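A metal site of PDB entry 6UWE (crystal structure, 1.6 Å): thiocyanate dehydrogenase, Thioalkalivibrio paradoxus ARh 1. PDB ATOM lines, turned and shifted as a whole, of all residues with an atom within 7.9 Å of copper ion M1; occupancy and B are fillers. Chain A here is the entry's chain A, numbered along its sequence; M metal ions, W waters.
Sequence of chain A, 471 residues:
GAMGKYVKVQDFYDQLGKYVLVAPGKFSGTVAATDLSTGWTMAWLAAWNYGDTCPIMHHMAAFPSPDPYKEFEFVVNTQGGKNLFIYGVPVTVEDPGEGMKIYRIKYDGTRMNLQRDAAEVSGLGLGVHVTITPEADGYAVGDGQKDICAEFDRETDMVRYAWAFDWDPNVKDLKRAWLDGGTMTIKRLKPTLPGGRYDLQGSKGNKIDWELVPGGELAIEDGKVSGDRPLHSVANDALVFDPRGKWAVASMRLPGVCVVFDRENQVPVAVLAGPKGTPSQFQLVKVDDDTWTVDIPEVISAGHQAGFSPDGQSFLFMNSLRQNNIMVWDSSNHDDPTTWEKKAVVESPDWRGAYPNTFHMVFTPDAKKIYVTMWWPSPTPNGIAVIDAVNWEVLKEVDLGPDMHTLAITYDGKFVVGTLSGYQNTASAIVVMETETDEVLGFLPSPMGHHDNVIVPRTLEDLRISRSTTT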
ATOM      1  N   HIS A  58      18.167  15.752  32.536  1.00  0.00           N
ATOM      2  CA  HIS A  58      18.267  14.459  31.816  1.00  0.00           C
ATOM      3  C   HIS A  58      19.587  13.716  32.117  1.00  0.00           C
ATOM      4  O   HIS A  58      19.554  12.748  32.867  1.00  0.00           O
ATOM      5  CB  HIS A  58      18.015  14.619  30.320  1.00  0.00           C
ATOM      6  CG  HIS A  58      17.740  13.306  29.665  1.00  0.00           C
ATOM      7  ND1 HIS A  58      17.780  13.120  28.310  1.00  0.00           N
ATOM      8  CD2 HIS A  58      17.370  12.129  30.206  1.00  0.00           C
ATOM      9  CE1 HIS A  58      17.444  11.858  28.033  1.00  0.00           C
ATOM     10  NE2 HIS A  58      17.254  11.232  29.175  1.00  0.00           N
ATOM     11  N   HIS A  59      20.690  14.128  31.521  1.00  0.00           N
ATOM     12  CA  HIS A  59      21.986  13.428  31.645  1.00  0.00           C
ATOM     13  C   HIS A  59      23.009  14.338  32.306  1.00  0.00           C
ATOM     14  O   HIS A  59      22.812  15.559  32.376  1.00  0.00           O
ATOM     15  CB  HIS A  59      22.414  12.857  30.301  1.00  0.00           C
ATOM     16  CG  HIS A  59      21.664  11.595  29.999  1.00  0.00           C
ATOM     17  ND1 HIS A  59      21.845  10.434  30.768  1.00  0.00           N
ATOM     18  CD2 HIS A  59      20.686  11.324  29.121  1.00  0.00           C
ATOM     19  CE1 HIS A  59      21.024   9.510  30.337  1.00  0.00           C
ATOM     20  NE2 HIS A  59      20.322  10.026  29.342  1.00  0.00           N
ATOM     21  N   VAL A 128      20.383  14.649  25.234  1.00  0.00           N
ATOM     22  CA  VAL A 128      20.584  13.239  25.658  1.00  0.00           C
ATOM     23  C   VAL A 128      21.966  13.117  26.332  1.00  0.00           C
ATOM     24  O   VAL A 128      22.218  13.909  27.267  1.00  0.00           O
ATOM     25  CB  VAL A 128      20.223  12.244  24.532  1.00  0.00           C
ATOM     26  CG1 VAL A 128      20.078  10.834  25.095  1.00  0.00           C
ATOM     27  CG2 VAL A 128      18.922  12.654  23.848  1.00  0.00           C
ATOM     28  N   HIS A 129      22.786  12.111  26.055  1.00  0.00           N
ATOM     29  CA  HIS A 129      23.914  11.773  26.957  1.00  0.00           C
ATOM     30  C   HIS A 129      24.945  12.892  27.006  1.00  0.00           C
ATOM     31  O   HIS A 129      25.257  13.454  25.968  1.00  0.00           O
ATOM     32  CB  HIS A 129      24.556  10.434  26.608  1.00  0.00           C
ATOM     33  CG  HIS A 129      23.666   9.306  26.999  1.00  0.00           C
ATOM     34  ND1 HIS A 129      23.640   8.805  28.254  1.00  0.00           N
ATOM     35  CD2 HIS A 129      22.757   8.620  26.281  1.00  0.00           C
ATOM     36  CE1 HIS A 129      22.749   7.832  28.298  1.00  0.00           C
ATOM     37  NE2 HIS A 129      22.262   7.680  27.112  1.00  0.00           N
ATOM     38  N   LEU A 212      12.578   9.121  21.845  1.00  0.00           N
ATOM     39  CA  LEU A 212      12.223   7.696  21.960  1.00  0.00           C
ATOM     40  C   LEU A 212      12.543   7.285  23.400  1.00  0.00           C
ATOM     41  O   LEU A 212      13.720   7.377  23.818  1.00  0.00           O
ATOM     42  CB  LEU A 212      12.994   6.882  20.919  1.00  0.00           C
ATOM     43  CG  LEU A 212      12.753   7.289  19.469  1.00  0.00           C
ATOM     44  CD1 LEU A 212      13.503   6.359  18.538  1.00  0.00           C
ATOM     45  CD2 LEU A 212      11.256   7.285  19.144  1.00  0.00           C
ATOM     46  N   PRO A 214      12.893   5.013  27.032  1.00  0.00           N
ATOM     47  CA  PRO A 214      13.536   3.717  27.288  1.00  0.00           C
ATOM     48  C   PRO A 214      12.613   2.571  26.871  1.00  0.00           C
ATOM     49  O   PRO A 214      11.452   2.577  27.263  1.00  0.00           O
ATOM     50  CB  PRO A 214      13.810   3.703  28.801  1.00  0.00           C
ATOM     51  CG  PRO A 214      13.849   5.191  29.179  1.00  0.00           C
ATOM     52  CD  PRO A 214      12.905   5.890  28.222  1.00  0.00           C
ATOM     53  N   GLU A 217      11.855   2.346  21.280  1.00  0.00           N
ATOM     54  CA  GLU A 217      12.430   2.615  19.921  1.00  0.00           C
ATOM     55  C   GLU A 217      11.404   2.327  18.827  1.00  0.00           C
ATOM     56  O   GLU A 217      11.438   3.074  17.822  1.00  0.00           O
ATOM     57  CB  GLU A 217      13.727   1.834  19.689  1.00  0.00           C
ATOM     58  CG  GLU A 217      14.945   2.451  20.364  1.00  0.00           C
ATOM     59  CD  GLU A 217      15.100   2.115  21.847  1.00  0.00           C
ATOM     60  OE1 GLU A 217      14.287   1.317  22.365  1.00  0.00           O
ATOM     61  OE2 GLU A 217      16.049   2.635  22.470  1.00  0.00           O
ATOM     62  N   ASN A 236      20.413   9.457  17.386  1.00  0.00           N
ATOM     63  CA  ASN A 236      21.722   9.558  18.079  1.00  0.00           C
ATOM     64  C   ASN A 236      21.440   9.608  19.588  1.00  0.00           C
ATOM     65  O   ASN A 236      20.392  10.191  19.997  1.00  0.00           O
ATOM     66  CB  ASN A 236      22.525  10.760  17.608  1.00  0.00           C
ATOM     67  CG  ASN A 236      23.776  10.965  18.438  1.00  0.00           C
ATOM     68  OD1 ASN A 236      23.892  11.996  19.124  1.00  0.00           O
ATOM     69  ND2 ASN A 236      24.718  10.006  18.423  1.00  0.00           N
ATOM     70  N   ASP A 237      22.318   9.022  20.386  1.00  0.00           N
ATOM     71  CA  ASP A 237      22.110   8.882  21.850  1.00  0.00           C
ATOM     72  C   ASP A 237      23.288   9.515  22.589  1.00  0.00           C
ATOM     73  O   ASP A 237      23.066  10.323  23.525  1.00  0.00           O
ATOM     74  CB  ASP A 237      21.869   7.407  22.180  1.00  0.00           C
ATOM     75  CG  ASP A 237      21.318   7.175  23.572  1.00  0.00           C
ATOM     76  OD1 ASP A 237      20.201   7.665  23.809  1.00  0.00           O
ATOM     77  OD2 ASP A 237      22.020   6.568  24.406  1.00  0.00           O
ATOM     78  N   ALA A 238      24.520   9.133  22.240  1.00  0.00           N
ATOM     79  CA  ALA A 238      25.712   9.485  23.026  1.00  0.00           C
ATOM     80  C   ALA A 238      26.917   9.599  22.092  1.00  0.00           C
ATOM     81  O   ALA A 238      26.878   9.118  20.962  1.00  0.00           O
ATOM     82  CB  ALA A 238      25.970   8.452  24.093  1.00  0.00           C
ATOM     83  N   SER A 251      26.684   6.671  19.109  1.00  0.00           N
ATOM     84  CA  SER A 251      25.689   5.571  19.062  1.00  0.00           C
ATOM     85  C   SER A 251      24.425   6.032  18.345  1.00  0.00           C
ATOM     86  O   SER A 251      23.930   7.128  18.657  1.00  0.00           O
ATOM     87  CB  SER A 251      25.425   5.059  20.453  1.00  0.00           C
ATOM     88  OG  SER A 251      25.119   6.122  21.325  1.00  0.00           O
ATOM     89  N   ARG A 253      20.605   4.728  17.612  1.00  0.00           N
ATOM     90  CA  ARG A 253      19.666   3.695  18.109  1.00  0.00           C
ATOM     91  C   ARG A 253      18.931   3.022  16.938  1.00  0.00           C
ATOM     92  O   ARG A 253      18.903   1.766  16.903  1.00  0.00           O
ATOM     93  CB  ARG A 253      18.669   4.289  19.120  1.00  0.00           C
ATOM     94  CG  ARG A 253      19.318   4.735  20.426  1.00  0.00           C
ATOM     95  CD  ARG A 253      18.413   5.688  21.211  1.00  0.00           C
ATOM     96  NE  ARG A 253      17.286   5.076  21.869  1.00  0.00           N
ATOM     97  CZ  ARG A 253      16.325   5.774  22.483  1.00  0.00           C
ATOM     98  NH1 ARG A 253      16.318   7.097  22.452  1.00  0.00           N
ATOM     99  NH2 ARG A 253      15.341   5.152  23.092  1.00  0.00           N
ATOM    100  N   GLY A 303      19.555  -0.558  18.677  1.00  0.00           N
ATOM    101  CA  GLY A 303      20.488  -0.666  19.797  1.00  0.00           C
ATOM    102  C   GLY A 303      20.405   0.578  20.644  1.00  0.00           C
ATOM    103  O   GLY A 303      19.636   1.487  20.276  1.00  0.00           O
ATOM    104  N   HIS A 304      21.099   0.607  21.767  1.00  0.00           N
ATOM    105  CA  HIS A 304      21.041   1.799  22.659  1.00  0.00           C
ATOM    106  C   HIS A 304      22.388   1.988  23.365  1.00  0.00           C
ATOM    107  O   HIS A 304      23.203   2.798  22.835  1.00  0.00           O
ATOM    108  CB  HIS A 304      19.827   1.748  23.596  1.00  0.00           C
ATOM    109  CG  HIS A 304      19.653   2.998  24.403  1.00  0.00           C
ATOM    110  ND1 HIS A 304      18.482   3.299  25.071  1.00  0.00           N
ATOM    111  CD2 HIS A 304      20.503   4.005  24.676  1.00  0.00           C
ATOM    112  CE1 HIS A 304      18.599   4.439  25.701  1.00  0.00           C
ATOM    113  NE2 HIS A 304      19.845   4.853  25.524  1.00  0.00           N
ATOM    114  N   GLN A 305      22.611   1.384  24.530  1.00  0.00           N
ATOM    115  CA  GLN A 305      23.743   1.801  25.407  1.00  0.00           C
ATOM    116  C   GLN A 305      25.064   1.364  24.747  1.00  0.00           C
ATOM    117  O   GLN A 305      25.075   0.411  23.921  1.00  0.00           O
ATOM    118  CB  GLN A 305      23.581   1.311  26.852  1.00  0.00           C
ATOM    119  CG  GLN A 305      22.270   1.677  27.551  1.00  0.00           C
ATOM    120  CD  GLN A 305      21.937   3.140  27.718  1.00  0.00           C
ATOM    121  OE1 GLN A 305      22.743   4.044  27.472  1.00  0.00           O
ATOM    122  NE2 GLN A 305      20.691   3.396  28.138  1.00  0.00           N
ATOM    123  N   ALA A 306      26.138   2.081  25.020  1.00  0.00           N
ATOM    124  CA  ALA A 306      27.447   1.843  24.396  1.00  0.00           C
ATOM    125  C   ALA A 306      28.561   2.201  25.375  1.00  0.00           C
ATOM    126  O   ALA A 306      28.367   3.077  26.278  1.00  0.00           O
ATOM    127  CB  ALA A 306      27.599   2.633  23.134  1.00  0.00           C
ATOM    128  N   PHE A 359      21.005  -2.773  29.272  1.00  0.00           N
ATOM    129  CA  PHE A 359      20.850  -1.297  29.444  1.00  0.00           C
ATOM    130  C   PHE A 359      22.207  -0.707  29.849  1.00  0.00           C
ATOM    131  O   PHE A 359      23.245  -1.040  29.224  1.00  0.00           O
ATOM    132  CB  PHE A 359      19.668  -1.060  30.408  1.00  0.00           C
ATOM    133  CG  PHE A 359      18.865   0.200  30.169  1.00  0.00           C
ATOM    134  CD1 PHE A 359      18.615   0.670  28.884  1.00  0.00           C
ATOM    135  CD2 PHE A 359      18.295   0.871  31.233  1.00  0.00           C
ATOM    136  CE1 PHE A 359      17.848   1.805  28.688  1.00  0.00           C
ATOM    137  CE2 PHE A 359      17.528   2.006  31.037  1.00  0.00           C
ATOM    138  CZ  PHE A 359      17.289   2.460  29.763  1.00  0.00           C
ATOM    139  N   HIS A 360      22.215   0.219  30.809  1.00  0.00           N
ATOM    140  CA  HIS A 360      23.418   0.968  31.233  1.00  0.00           C
ATOM    141  C   HIS A 360      24.464   0.026  31.822  1.00  0.00           C
ATOM    142  O   HIS A 360      24.119  -1.091  32.239  1.00  0.00           O
ATOM    143  CB  HIS A 360      23.060   2.016  32.256  1.00  0.00           C
ATOM    144  CG  HIS A 360      22.115   3.037  31.743  1.00  0.00           C
ATOM    145  ND1 HIS A 360      22.544   4.154  31.019  1.00  0.00           N
ATOM    146  CD2 HIS A 360      20.781   3.173  31.886  1.00  0.00           C
ATOM    147  CE1 HIS A 360      21.521   4.904  30.739  1.00  0.00           C
ATOM    148  NE2 HIS A 360      20.437   4.340  31.281  1.00  0.00           N
ATOM    149  N   HIS A 405      17.981   2.526  35.813  1.00  0.00           N
ATOM    150  CA  HIS A 405      18.791   3.302  34.840  1.00  0.00           C
ATOM    151  C   HIS A 405      20.277   3.047  35.091  1.00  0.00           C
ATOM    152  O   HIS A 405      20.740   1.904  34.841  1.00  0.00           O
ATOM    153  CB  HIS A 405      18.340   4.785  34.868  1.00  0.00           C
ATOM    154  CG  HIS A 405      17.049   4.926  34.128  1.00  0.00           C
ATOM    155  ND1 HIS A 405      16.987   5.127  32.774  1.00  0.00           N
ATOM    156  CD2 HIS A 405      15.793   4.669  34.529  1.00  0.00           C
ATOM    157  CE1 HIS A 405      15.717   5.146  32.394  1.00  0.00           C
ATOM    158  NE2 HIS A 405      14.974   4.838  33.446  1.00  0.00           N
ATOM    159  N   THR A 406      21.022   4.074  35.457  1.00  0.00           N
ATOM    160  CA  THR A 406      22.497   4.027  35.384  1.00  0.00           C
ATOM    161  C   THR A 406      23.110   3.345  36.598  1.00  0.00           C
ATOM    162  O   THR A 406      22.458   3.195  37.645  1.00  0.00           O
ATOM    163  CB  THR A 406      23.041   5.453  35.192  1.00  0.00           C
ATOM    164  OG1 THR A 406      22.252   6.258  36.074  1.00  0.00           O
ATOM    165  CG2 THR A 406      22.927   5.903  33.749  1.00  0.00           C
ATOM    166  N   HIS A 451      17.753   9.389  35.121  1.00  0.00           N
ATOM    167  CA  HIS A 451      18.268   8.573  33.993  1.00  0.00           C
ATOM    168  C   HIS A 451      19.800   8.583  34.006  1.00  0.00           C
ATOM    169  O   HIS A 451      20.390   8.099  33.046  1.00  0.00           O
ATOM    170  CB  HIS A 451      17.711   9.073  32.664  1.00  0.00           C
ATOM    171  CG  HIS A 451      16.282   8.730  32.459  1.00  0.00           C
ATOM    172  ND1 HIS A 451      15.699   8.737  31.193  1.00  0.00           N
ATOM    173  CD2 HIS A 451      15.343   8.308  33.329  1.00  0.00           C
ATOM    174  CE1 HIS A 451      14.434   8.389  31.323  1.00  0.00           C
ATOM    175  NE2 HIS A 451      14.193   8.107  32.617  1.00  0.00           N
ATOM    176  N   THR A 471      27.876   4.931  28.715  1.00  0.00           N
ATOM    177  CA  THR A 471      26.555   5.399  29.177  1.00  0.00           C
ATOM    178  C   THR A 471      26.112   4.522  30.358  1.00  0.00           C
ATOM    179  O   THR A 471      25.133   4.864  31.015  1.00  0.00           O
ATOM    180  CB  THR A 471      25.545   5.375  28.024  1.00  0.00           C
ATOM    181  OG1 THR A 471      25.353   4.030  27.586  1.00  0.00           O
ATOM    182  CG2 THR A 471      25.965   6.229  26.839  1.00  0.00           C
ATOM    183  OXT THR A 471      26.718   3.480  30.666  1.00  0.00           O
HETATM  184 CU    CU M   1      21.018   6.349  26.235  1.00  0.00          CU
HETATM  185 CU    CU M   2      19.027   8.814  28.445  1.00  0.00          CU
HETATM  186 CU    CU M   3      18.593   5.076  31.675  1.00  0.00          CU
HETATM  187 CU    CU M   4      16.641   9.305  29.477  1.00  0.00          CU
HETATM  188  O   HOH W   1      18.125   8.141  25.585  1.00  0.00           O
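Copper ion M1 is bound by a ring nitrogen (NE2) of His 129 (2.0 Å), a ring nitrogen (NE2) of His 304 (2.0 Å) and the side-chain carboxylate of Asp 237 (2.1 Å).
Residues that only touch copper ion M1: Gln 305 (3.1 Å).
Of the 22 residues printed, 4 come within 4 Å of copper ion M1.
Along chain A the residues within 4 Å of copper ion M1 span positions 129 to 305.
OE1 of Gln 305 lies within hydrogen-bond range of OG1 of Thr 471 (2.6 Å).
NE2 of His 304 lies close to NE2 of Gln 305 (3.1 Å).
A ring nitrogen (ND1) of His 129 lies close to a ring nitrogen (ND1) of His 59, 3.5 Å away.
The side-chain amide nitrogen of Gln 305 sits close to a ring nitrogen (NE2) of His 360 (3.3 Å).
The backbone NH (N) of Asp 237 sits at hydrogen-bond distance from the backbone carbonyl oxygen (O) of Ser 251.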
